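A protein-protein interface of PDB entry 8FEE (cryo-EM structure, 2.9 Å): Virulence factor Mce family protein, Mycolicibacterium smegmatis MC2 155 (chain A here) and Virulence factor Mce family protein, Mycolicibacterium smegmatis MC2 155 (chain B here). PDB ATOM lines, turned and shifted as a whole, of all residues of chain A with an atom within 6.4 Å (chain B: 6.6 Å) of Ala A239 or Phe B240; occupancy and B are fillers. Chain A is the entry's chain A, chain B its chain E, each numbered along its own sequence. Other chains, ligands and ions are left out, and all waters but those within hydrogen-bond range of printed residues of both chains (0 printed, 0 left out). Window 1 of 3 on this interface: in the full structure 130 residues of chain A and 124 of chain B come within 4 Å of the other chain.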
ATOM      1  N   ASP A 234     -18.878  19.356 -27.108  1.00  0.00           N
ATOM      2  CA  ASP A 234     -18.356  20.073 -28.271  1.00  0.00           C
ATOM      3  C   ASP A 234     -17.258  21.049 -27.857  1.00  0.00           C
ATOM      4  O   ASP A 234     -16.209  21.151 -28.520  1.00  0.00           O
ATOM      5  CB  ASP A 234     -19.486  20.806 -28.991  1.00  0.00           C
ATOM      6  CG  ASP A 234     -20.528  19.861 -29.549  1.00  0.00           C
ATOM      7  OD1 ASP A 234     -20.360  18.633 -29.395  1.00  0.00           O
ATOM      8  OD2 ASP A 234     -21.516  20.343 -30.140  1.00  0.00           O
ATOM      9  N   GLY A 235     -17.484  21.772 -26.755  1.00  0.00           N
ATOM     10  CA  GLY A 235     -16.452  22.639 -26.229  1.00  0.00           C
ATOM     11  C   GLY A 235     -15.209  21.877 -25.829  1.00  0.00           C
ATOM     12  O   GLY A 235     -14.099  22.377 -25.986  1.00  0.00           O
ATOM     13  N   LEU A 236     -15.374  20.652 -25.325  1.00  0.00           N
ATOM     14  CA  LEU A 236     -14.220  19.842 -24.955  1.00  0.00           C
ATOM     15  C   LEU A 236     -13.461  19.366 -26.185  1.00  0.00           C
ATOM     16  O   LEU A 236     -12.233  19.290 -26.160  1.00  0.00           O
ATOM     17  CB  LEU A 236     -14.652  18.655 -24.095  1.00  0.00           C
ATOM     18  CG  LEU A 236     -14.961  18.953 -22.627  1.00  0.00           C
ATOM     19  CD1 LEU A 236     -15.175  17.665 -21.852  1.00  0.00           C
ATOM     20  CD2 LEU A 236     -13.851  19.782 -22.003  1.00  0.00           C
ATOM     21  N   ASP A 237     -14.169  19.047 -27.272  1.00  0.00           N
ATOM     22  CA  ASP A 237     -13.492  18.704 -28.524  1.00  0.00           C
ATOM     23  C   ASP A 237     -12.615  19.856 -29.002  1.00  0.00           C
ATOM     24  O   ASP A 237     -11.413  19.686 -29.268  1.00  0.00           O
ATOM     25  CB  ASP A 237     -14.520  18.347 -29.599  1.00  0.00           C
ATOM     26  CG  ASP A 237     -14.724  16.856 -29.743  1.00  0.00           C
ATOM     27  OD1 ASP A 237     -13.747  16.102 -29.557  1.00  0.00           O
ATOM     28  OD2 ASP A 237     -15.859  16.438 -30.047  1.00  0.00           O
ATOM     29  N   ASN A 238     -13.203  21.044 -29.113  1.00  0.00           N
ATOM     30  CA  ASN A 238     -12.430  22.169 -29.628  1.00  0.00           C
ATOM     31  C   ASN A 238     -11.370  22.627 -28.627  1.00  0.00           C
ATOM     32  O   ASN A 238     -10.295  23.100 -29.027  1.00  0.00           O
ATOM     33  CB  ASN A 238     -13.376  23.298 -30.013  1.00  0.00           C
ATOM     34  CG  ASN A 238     -14.340  22.889 -31.110  1.00  0.00           C
ATOM     35  OD1 ASN A 238     -14.008  22.074 -31.969  1.00  0.00           O
ATOM     36  ND2 ASN A 238     -15.549  23.436 -31.072  1.00  0.00           N
ATOM     37  N   ALA A 239     -11.633  22.462 -27.329  1.00  0.00           N
ATOM     38  CA  ALA A 239     -10.626  22.732 -26.316  1.00  0.00           C
ATOM     39  C   ALA A 239      -9.490  21.727 -26.386  1.00  0.00           C
ATOM     40  O   ALA A 239      -8.351  22.069 -26.074  1.00  0.00           O
ATOM     41  CB  ALA A 239     -11.264  22.729 -24.929  1.00  0.00           C
ATOM     42  N   VAL A 240      -9.774  20.493 -26.801  1.00  0.00           N
ATOM     43  CA  VAL A 240      -8.716  19.515 -27.028  1.00  0.00           C
ATOM     44  C   VAL A 240      -7.848  19.948 -28.197  1.00  0.00           C
ATOM     45  O   VAL A 240      -6.617  19.834 -28.148  1.00  0.00           O
ATOM     46  CB  VAL A 240      -9.321  18.116 -27.248  1.00  0.00           C
ATOM     47  CG1 VAL A 240      -8.350  17.215 -27.972  1.00  0.00           C
ATOM     48  CG2 VAL A 240      -9.661  17.497 -25.923  1.00  0.00           C
ATOM     49  N   THR A 241      -8.473  20.438 -29.268  1.00  0.00           N
ATOM     50  CA  THR A 241      -7.694  20.946 -30.399  1.00  0.00           C
ATOM     51  C   THR A 241      -6.770  22.089 -29.970  1.00  0.00           C
ATOM     52  O   THR A 241      -5.555  22.056 -30.224  1.00  0.00           O
ATOM     53  CB  THR A 241      -8.631  21.401 -31.519  1.00  0.00           C
ATOM     54  OG1 THR A 241      -9.187  20.256 -32.174  1.00  0.00           O
ATOM     55  CG2 THR A 241      -7.877  22.241 -32.538  1.00  0.00           C
ATOM     56  N   THR A 242      -7.322  23.099 -29.293  1.00  0.00           N
ATOM     57  CA  THR A 242      -6.472  24.208 -28.858  1.00  0.00           C
ATOM     58  C   THR A 242      -5.494  23.799 -27.757  1.00  0.00           C
ATOM     59  O   THR A 242      -4.434  24.418 -27.632  1.00  0.00           O
ATOM     60  CB  THR A 242      -7.310  25.407 -28.404  1.00  0.00           C
ATOM     61  OG1 THR A 242      -6.441  26.512 -28.130  1.00  0.00           O
ATOM     62  CG2 THR A 242      -8.085  25.091 -27.152  1.00  0.00           C
ATOM     63  N   ALA A 243      -5.798  22.752 -26.988  1.00  0.00           N
ATOM     64  CA  ALA A 243      -4.860  22.261 -25.986  1.00  0.00           C
ATOM     65  C   ALA A 243      -3.690  21.548 -26.642  1.00  0.00           C
ATOM     66  O   ALA A 243      -2.552  21.653 -26.175  1.00  0.00           O
ATOM     67  CB  ALA A 243      -5.576  21.334 -25.006  1.00  0.00           C
ATOM     68  N   ARG A 244      -3.955  20.812 -27.721  1.00  0.00           N
ATOM     69  CA  ARG A 244      -2.875  20.243 -28.515  1.00  0.00           C
ATOM     70  C   ARG A 244      -1.995  21.347 -29.079  1.00  0.00           C
ATOM     71  O   ARG A 244      -0.760  21.250 -29.046  1.00  0.00           O
ATOM     72  CB  ARG A 244      -3.448  19.382 -29.640  1.00  0.00           C
ATOM     73  CG  ARG A 244      -2.410  18.824 -30.593  1.00  0.00           C
ATOM     74  CD  ARG A 244      -3.070  18.115 -31.763  1.00  0.00           C
ATOM     75  NE  ARG A 244      -3.976  17.061 -31.325  1.00  0.00           N
ATOM     76  CZ  ARG A 244      -3.642  15.782 -31.220  1.00  0.00           C
ATOM     77  NH1 ARG A 244      -2.423  15.360 -31.512  1.00  0.00           N
ATOM     78  NH2 ARG A 244      -4.555  14.904 -30.814  1.00  0.00           N
ATOM     79  N   ASN A 247       0.096  22.709 -26.277  1.00  0.00           N
ATOM     80  CA  ASN A 247       1.133  21.755 -25.898  1.00  0.00           C
ATOM     81  C   ASN A 247       2.290  21.762 -26.888  1.00  0.00           C
ATOM     82  O   ASN A 247       3.457  21.673 -26.487  1.00  0.00           O
ATOM     83  CB  ASN A 247       0.537  20.352 -25.784  1.00  0.00           C
ATOM     84  CG  ASN A 247      -0.322  20.185 -24.549  1.00  0.00           C
ATOM     85  OD1 ASN A 247      -0.088  20.827 -23.527  1.00  0.00           O
ATOM     86  ND2 ASN A 247      -1.324  19.318 -24.638  1.00  0.00           N
ATOM     87  N   ARG B 235     -10.050  11.876 -25.726  1.00  0.00           N
ATOM     88  CA  ARG B 235      -9.165  12.946 -26.180  1.00  0.00           C
ATOM     89  C   ARG B 235      -8.839  13.909 -25.043  1.00  0.00           C
ATOM     90  O   ARG B 235      -7.682  14.324 -24.881  1.00  0.00           O
ATOM     91  CB  ARG B 235      -9.801  13.686 -27.357  1.00  0.00           C
ATOM     92  CG  ARG B 235      -9.775  12.901 -28.658  1.00  0.00           C
ATOM     93  CD  ARG B 235     -10.757  13.459 -29.675  1.00  0.00           C
ATOM     94  NE  ARG B 235     -10.645  14.904 -29.824  1.00  0.00           N
ATOM     95  CZ  ARG B 235      -9.992  15.508 -30.808  1.00  0.00           C
ATOM     96  NH1 ARG B 235      -9.370  14.818 -31.749  1.00  0.00           N
ATOM     97  NH2 ARG B 235      -9.969  16.837 -30.853  1.00  0.00           N
ATOM     98  N   VAL B 236      -9.850  14.282 -24.251  1.00  0.00           N
ATOM     99  CA  VAL B 236      -9.627  15.167 -23.110  1.00  0.00           C
ATOM    100  C   VAL B 236      -8.645  14.532 -22.135  1.00  0.00           C
ATOM    101  O   VAL B 236      -7.664  15.158 -21.715  1.00  0.00           O
ATOM    102  CB  VAL B 236     -10.962  15.500 -22.417  1.00  0.00           C
ATOM    103  CG1 VAL B 236     -10.709  16.206 -21.096  1.00  0.00           C
ATOM    104  CG2 VAL B 236     -11.833  16.363 -23.305  1.00  0.00           C
ATOM    105  N   LEU B 237      -8.889  13.268 -21.777  1.00  0.00           N
ATOM    106  CA  LEU B 237      -8.023  12.592 -20.816  1.00  0.00           C
ATOM    107  C   LEU B 237      -6.600  12.423 -21.338  1.00  0.00           C
ATOM    108  O   LEU B 237      -5.650  12.412 -20.547  1.00  0.00           O
ATOM    109  CB  LEU B 237      -8.621  11.237 -20.439  1.00  0.00           C
ATOM    110  CG  LEU B 237      -9.852  11.300 -19.534  1.00  0.00           C
ATOM    111  CD1 LEU B 237     -10.438   9.917 -19.315  1.00  0.00           C
ATOM    112  CD2 LEU B 237      -9.492  11.947 -18.209  1.00  0.00           C
ATOM    113  N   THR B 238      -6.426  12.292 -22.655  1.00  0.00           N
ATOM    114  CA  THR B 238      -5.075  12.219 -23.208  1.00  0.00           C
ATOM    115  C   THR B 238      -4.368  13.567 -23.169  1.00  0.00           C
ATOM    116  O   THR B 238      -3.193  13.644 -22.789  1.00  0.00           O
ATOM    117  CB  THR B 238      -5.106  11.704 -24.649  1.00  0.00           C
ATOM    118  OG1 THR B 238      -6.043  12.469 -25.415  1.00  0.00           O
ATOM    119  CG2 THR B 238      -5.480  10.237 -24.700  1.00  0.00           C
ATOM    120  N   GLU B 239      -5.058  14.643 -23.550  1.00  0.00           N
ATOM    121  CA  GLU B 239      -4.356  15.880 -23.873  1.00  0.00           C
ATOM    122  C   GLU B 239      -4.377  16.937 -22.778  1.00  0.00           C
ATOM    123  O   GLU B 239      -3.484  17.792 -22.761  1.00  0.00           O
ATOM    124  CB  GLU B 239      -4.913  16.474 -25.171  1.00  0.00           C
ATOM    125  CG  GLU B 239      -4.963  15.459 -26.302  1.00  0.00           C
ATOM    126  CD  GLU B 239      -5.141  16.099 -27.658  1.00  0.00           C
ATOM    127  OE1 GLU B 239      -5.050  17.340 -27.745  1.00  0.00           O
ATOM    128  OE2 GLU B 239      -5.376  15.360 -28.639  1.00  0.00           O
ATOM    129  N   PHE B 240      -5.350  16.922 -21.871  1.00  0.00           N
ATOM    130  CA  PHE B 240      -5.435  17.989 -20.876  1.00  0.00           C
ATOM    131  C   PHE B 240      -4.527  17.830 -19.651  1.00  0.00           C
ATOM    132  O   PHE B 240      -4.008  18.850 -19.178  1.00  0.00           O
ATOM    133  CB  PHE B 240      -6.886  18.165 -20.425  1.00  0.00           C
ATOM    134  CG  PHE B 240      -7.653  19.151 -21.253  1.00  0.00           C
ATOM    135  CD1 PHE B 240      -7.502  20.511 -21.042  1.00  0.00           C
ATOM    136  CD2 PHE B 240      -8.510  18.724 -22.248  1.00  0.00           C
ATOM    137  CE1 PHE B 240      -8.200  21.423 -21.800  1.00  0.00           C
ATOM    138  CE2 PHE B 240      -9.213  19.632 -23.011  1.00  0.00           C
ATOM    139  CZ  PHE B 240      -9.056  20.983 -22.786  1.00  0.00           C
ATOM    140  N   PRO B 241      -4.346  16.638 -19.071  1.00  0.00           N
ATOM    141  CA  PRO B 241      -3.479  16.522 -17.876  1.00  0.00           C
ATOM    142  C   PRO B 241      -2.067  17.053 -18.095  1.00  0.00           C
ATOM    143  O   PRO B 241      -1.533  17.711 -17.189  1.00  0.00           O
ATOM    144  CB  PRO B 241      -3.478  15.013 -17.586  1.00  0.00           C
ATOM    145  CG  PRO B 241      -4.802  14.575 -18.037  1.00  0.00           C
ATOM    146  CD  PRO B 241      -5.112  15.388 -19.267  1.00  0.00           C
ATOM    147  N   PRO B 242      -1.406  16.797 -19.245  1.00  0.00           N
ATOM    148  CA  PRO B 242      -0.084  17.427 -19.433  1.00  0.00           C
ATOM    149  C   PRO B 242      -0.141  18.943 -19.435  1.00  0.00           C
ATOM    150  O   PRO B 242       0.735  19.600 -18.855  1.00  0.00           O
ATOM    151  CB  PRO B 242       0.386  16.874 -20.786  1.00  0.00           C
ATOM    152  CG  PRO B 242      -0.368  15.634 -20.972  1.00  0.00           C
ATOM    153  CD  PRO B 242      -1.704  15.892 -20.374  1.00  0.00           C
ATOM    154  N   LEU B 243      -1.163  19.516 -20.075  1.00  0.00           N
ATOM    155  CA  LEU B 243      -1.308  20.967 -20.112  1.00  0.00           C
ATOM    156  C   LEU B 243      -1.509  21.530 -18.712  1.00  0.00           C
ATOM    157  O   LEU B 243      -0.913  22.552 -18.351  1.00  0.00           O
ATOM    158  CB  LEU B 243      -2.475  21.351 -21.020  1.00  0.00           C
ATOM    159  CG  LEU B 243      -2.793  22.842 -21.123  1.00  0.00           C
ATOM    160  CD1 LEU B 243      -1.570  23.597 -21.605  1.00  0.00           C
ATOM    161  CD2 LEU B 243      -3.970  23.076 -22.052  1.00  0.00           C
ATOM    162  N   ILE B 244      -2.353  20.876 -17.911  1.00  0.00           N
ATOM    163  CA  ILE B 244      -2.636  21.365 -16.567  1.00  0.00           C
ATOM    164  C   ILE B 244      -1.403  21.232 -15.681  1.00  0.00           C
ATOM    165  O   ILE B 244      -1.116  22.111 -14.858  1.00  0.00           O
ATOM    166  CB  ILE B 244      -3.852  20.626 -15.980  1.00  0.00           C
ATOM    167  CG1 ILE B 244      -5.088  20.891 -16.838  1.00  0.00           C
ATOM    168  CG2 ILE B 244      -4.110  21.058 -14.549  1.00  0.00           C
ATOM    169  CD1 ILE B 244      -6.341  20.219 -16.332  1.00  0.00           C
ATOM    170  N   GLN B 245      -0.645  20.143 -15.843  1.00  0.00           N
ATOM    171  CA  GLN B 245       0.609  19.998 -15.109  1.00  0.00           C
ATOM    172  C   GLN B 245       1.592  21.101 -15.481  1.00  0.00           C
ATOM    173  O   GLN B 245       2.238  21.690 -14.604  1.00  0.00           O
ATOM    174  CB  GLN B 245       1.218  18.622 -15.377  1.00  0.00           C
ATOM    175  CG  GLN B 245       2.608  18.434 -14.795  1.00  0.00           C
ATOM    176  CD  GLN B 245       3.169  17.052 -15.067  1.00  0.00           C
ATOM    177  OE1 GLN B 245       2.698  16.342 -15.953  1.00  0.00           O
ATOM    178  NE2 GLN B 245       4.180  16.664 -14.299  1.00  0.00           N
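Hydrophobic or aromatic side chains of chain B that line the printed part of chain A: Val B236, Phe B240 and Leu B243. Along chain B the printed residues that touch a printed residue of chain A span positions 235 to 243. Along chain A the printed residues that touch a printed residue of chain B span positions 236 to 247. Among the printed residues, 12 pairs touch across the chains. Among the printed residues, Asp or Glu carboxylates within 4 Å of a Lys or Arg side-chain nitrogen of the other chain: Asp A237 with Arg B235 (3.3 Å) and Arg A244 with Glu B239 (2.4 Å).
The backbone carbonyl oxygen (O) of Val A240 lies close to the side-chain carboxylate (OE1) of Glu B239. The backbone carbonyl oxygen of Glu B239 lies within hydrogen-bond range of the side-chain amide nitrogen of Asn A247. NE of Arg A244 is in salt-bridge range of OE2 of Glu B239, at 3.5 Å. The side-chain carboxylate (OD1) of Asp A237 is in salt-bridge range of the guanidinium group (NE) of Arg B235 (3.3 Å).
The backbone carbonyl oxygen (O) of Ala A243 lies within hydrogen-bond range of the side-chain amide nitrogen (ND2) of Asn A247. The backbone carbonyl oxygen of Arg B235 lies within hydrogen-bond range of the side-chain hydroxyl of Thr B238.
Among the printed residues, merely in contact across the chains: Leu A236 with Val B236 (3.7 Å), Ala A239 with Phe B240 (3.5 Å), Val A240 with Arg B235 (3.3 Å), Val A240 with Val B236 (3.6 Å), Val A240 with Phe B240 (3.6 Å), Thr A241 with Arg B235 (3.7 Å), Ala A243 with Leu B243 (3.8 Å) and Asn A247 with Leu B243 (3.5 Å).
Of chain B, only Phe B240 (3.5 Å) comes within 4 Å of Ala A239. Of the printed residues of chain B, Leu A236 touches Val B236 (3.7 Å). Of the printed residues of chain A, Glu B239 touches Val A240, Arg A244 and Asn A247. Of the printed residues of chain B, Asn A247 touches Glu B239 and Leu B243. Of the printed residues of chain B, Ala A243 touches Leu B243. Printed residues of chain B within 4 Å of Thr A241: Arg B235 (3.7 Å). The nearest printed residue of chain B that does not touch Ala A239 is Glu B239 (6.0 Å). The nearest printed residue of chain B that does not touch Thr A241 is Glu B239 (4.9 Å).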
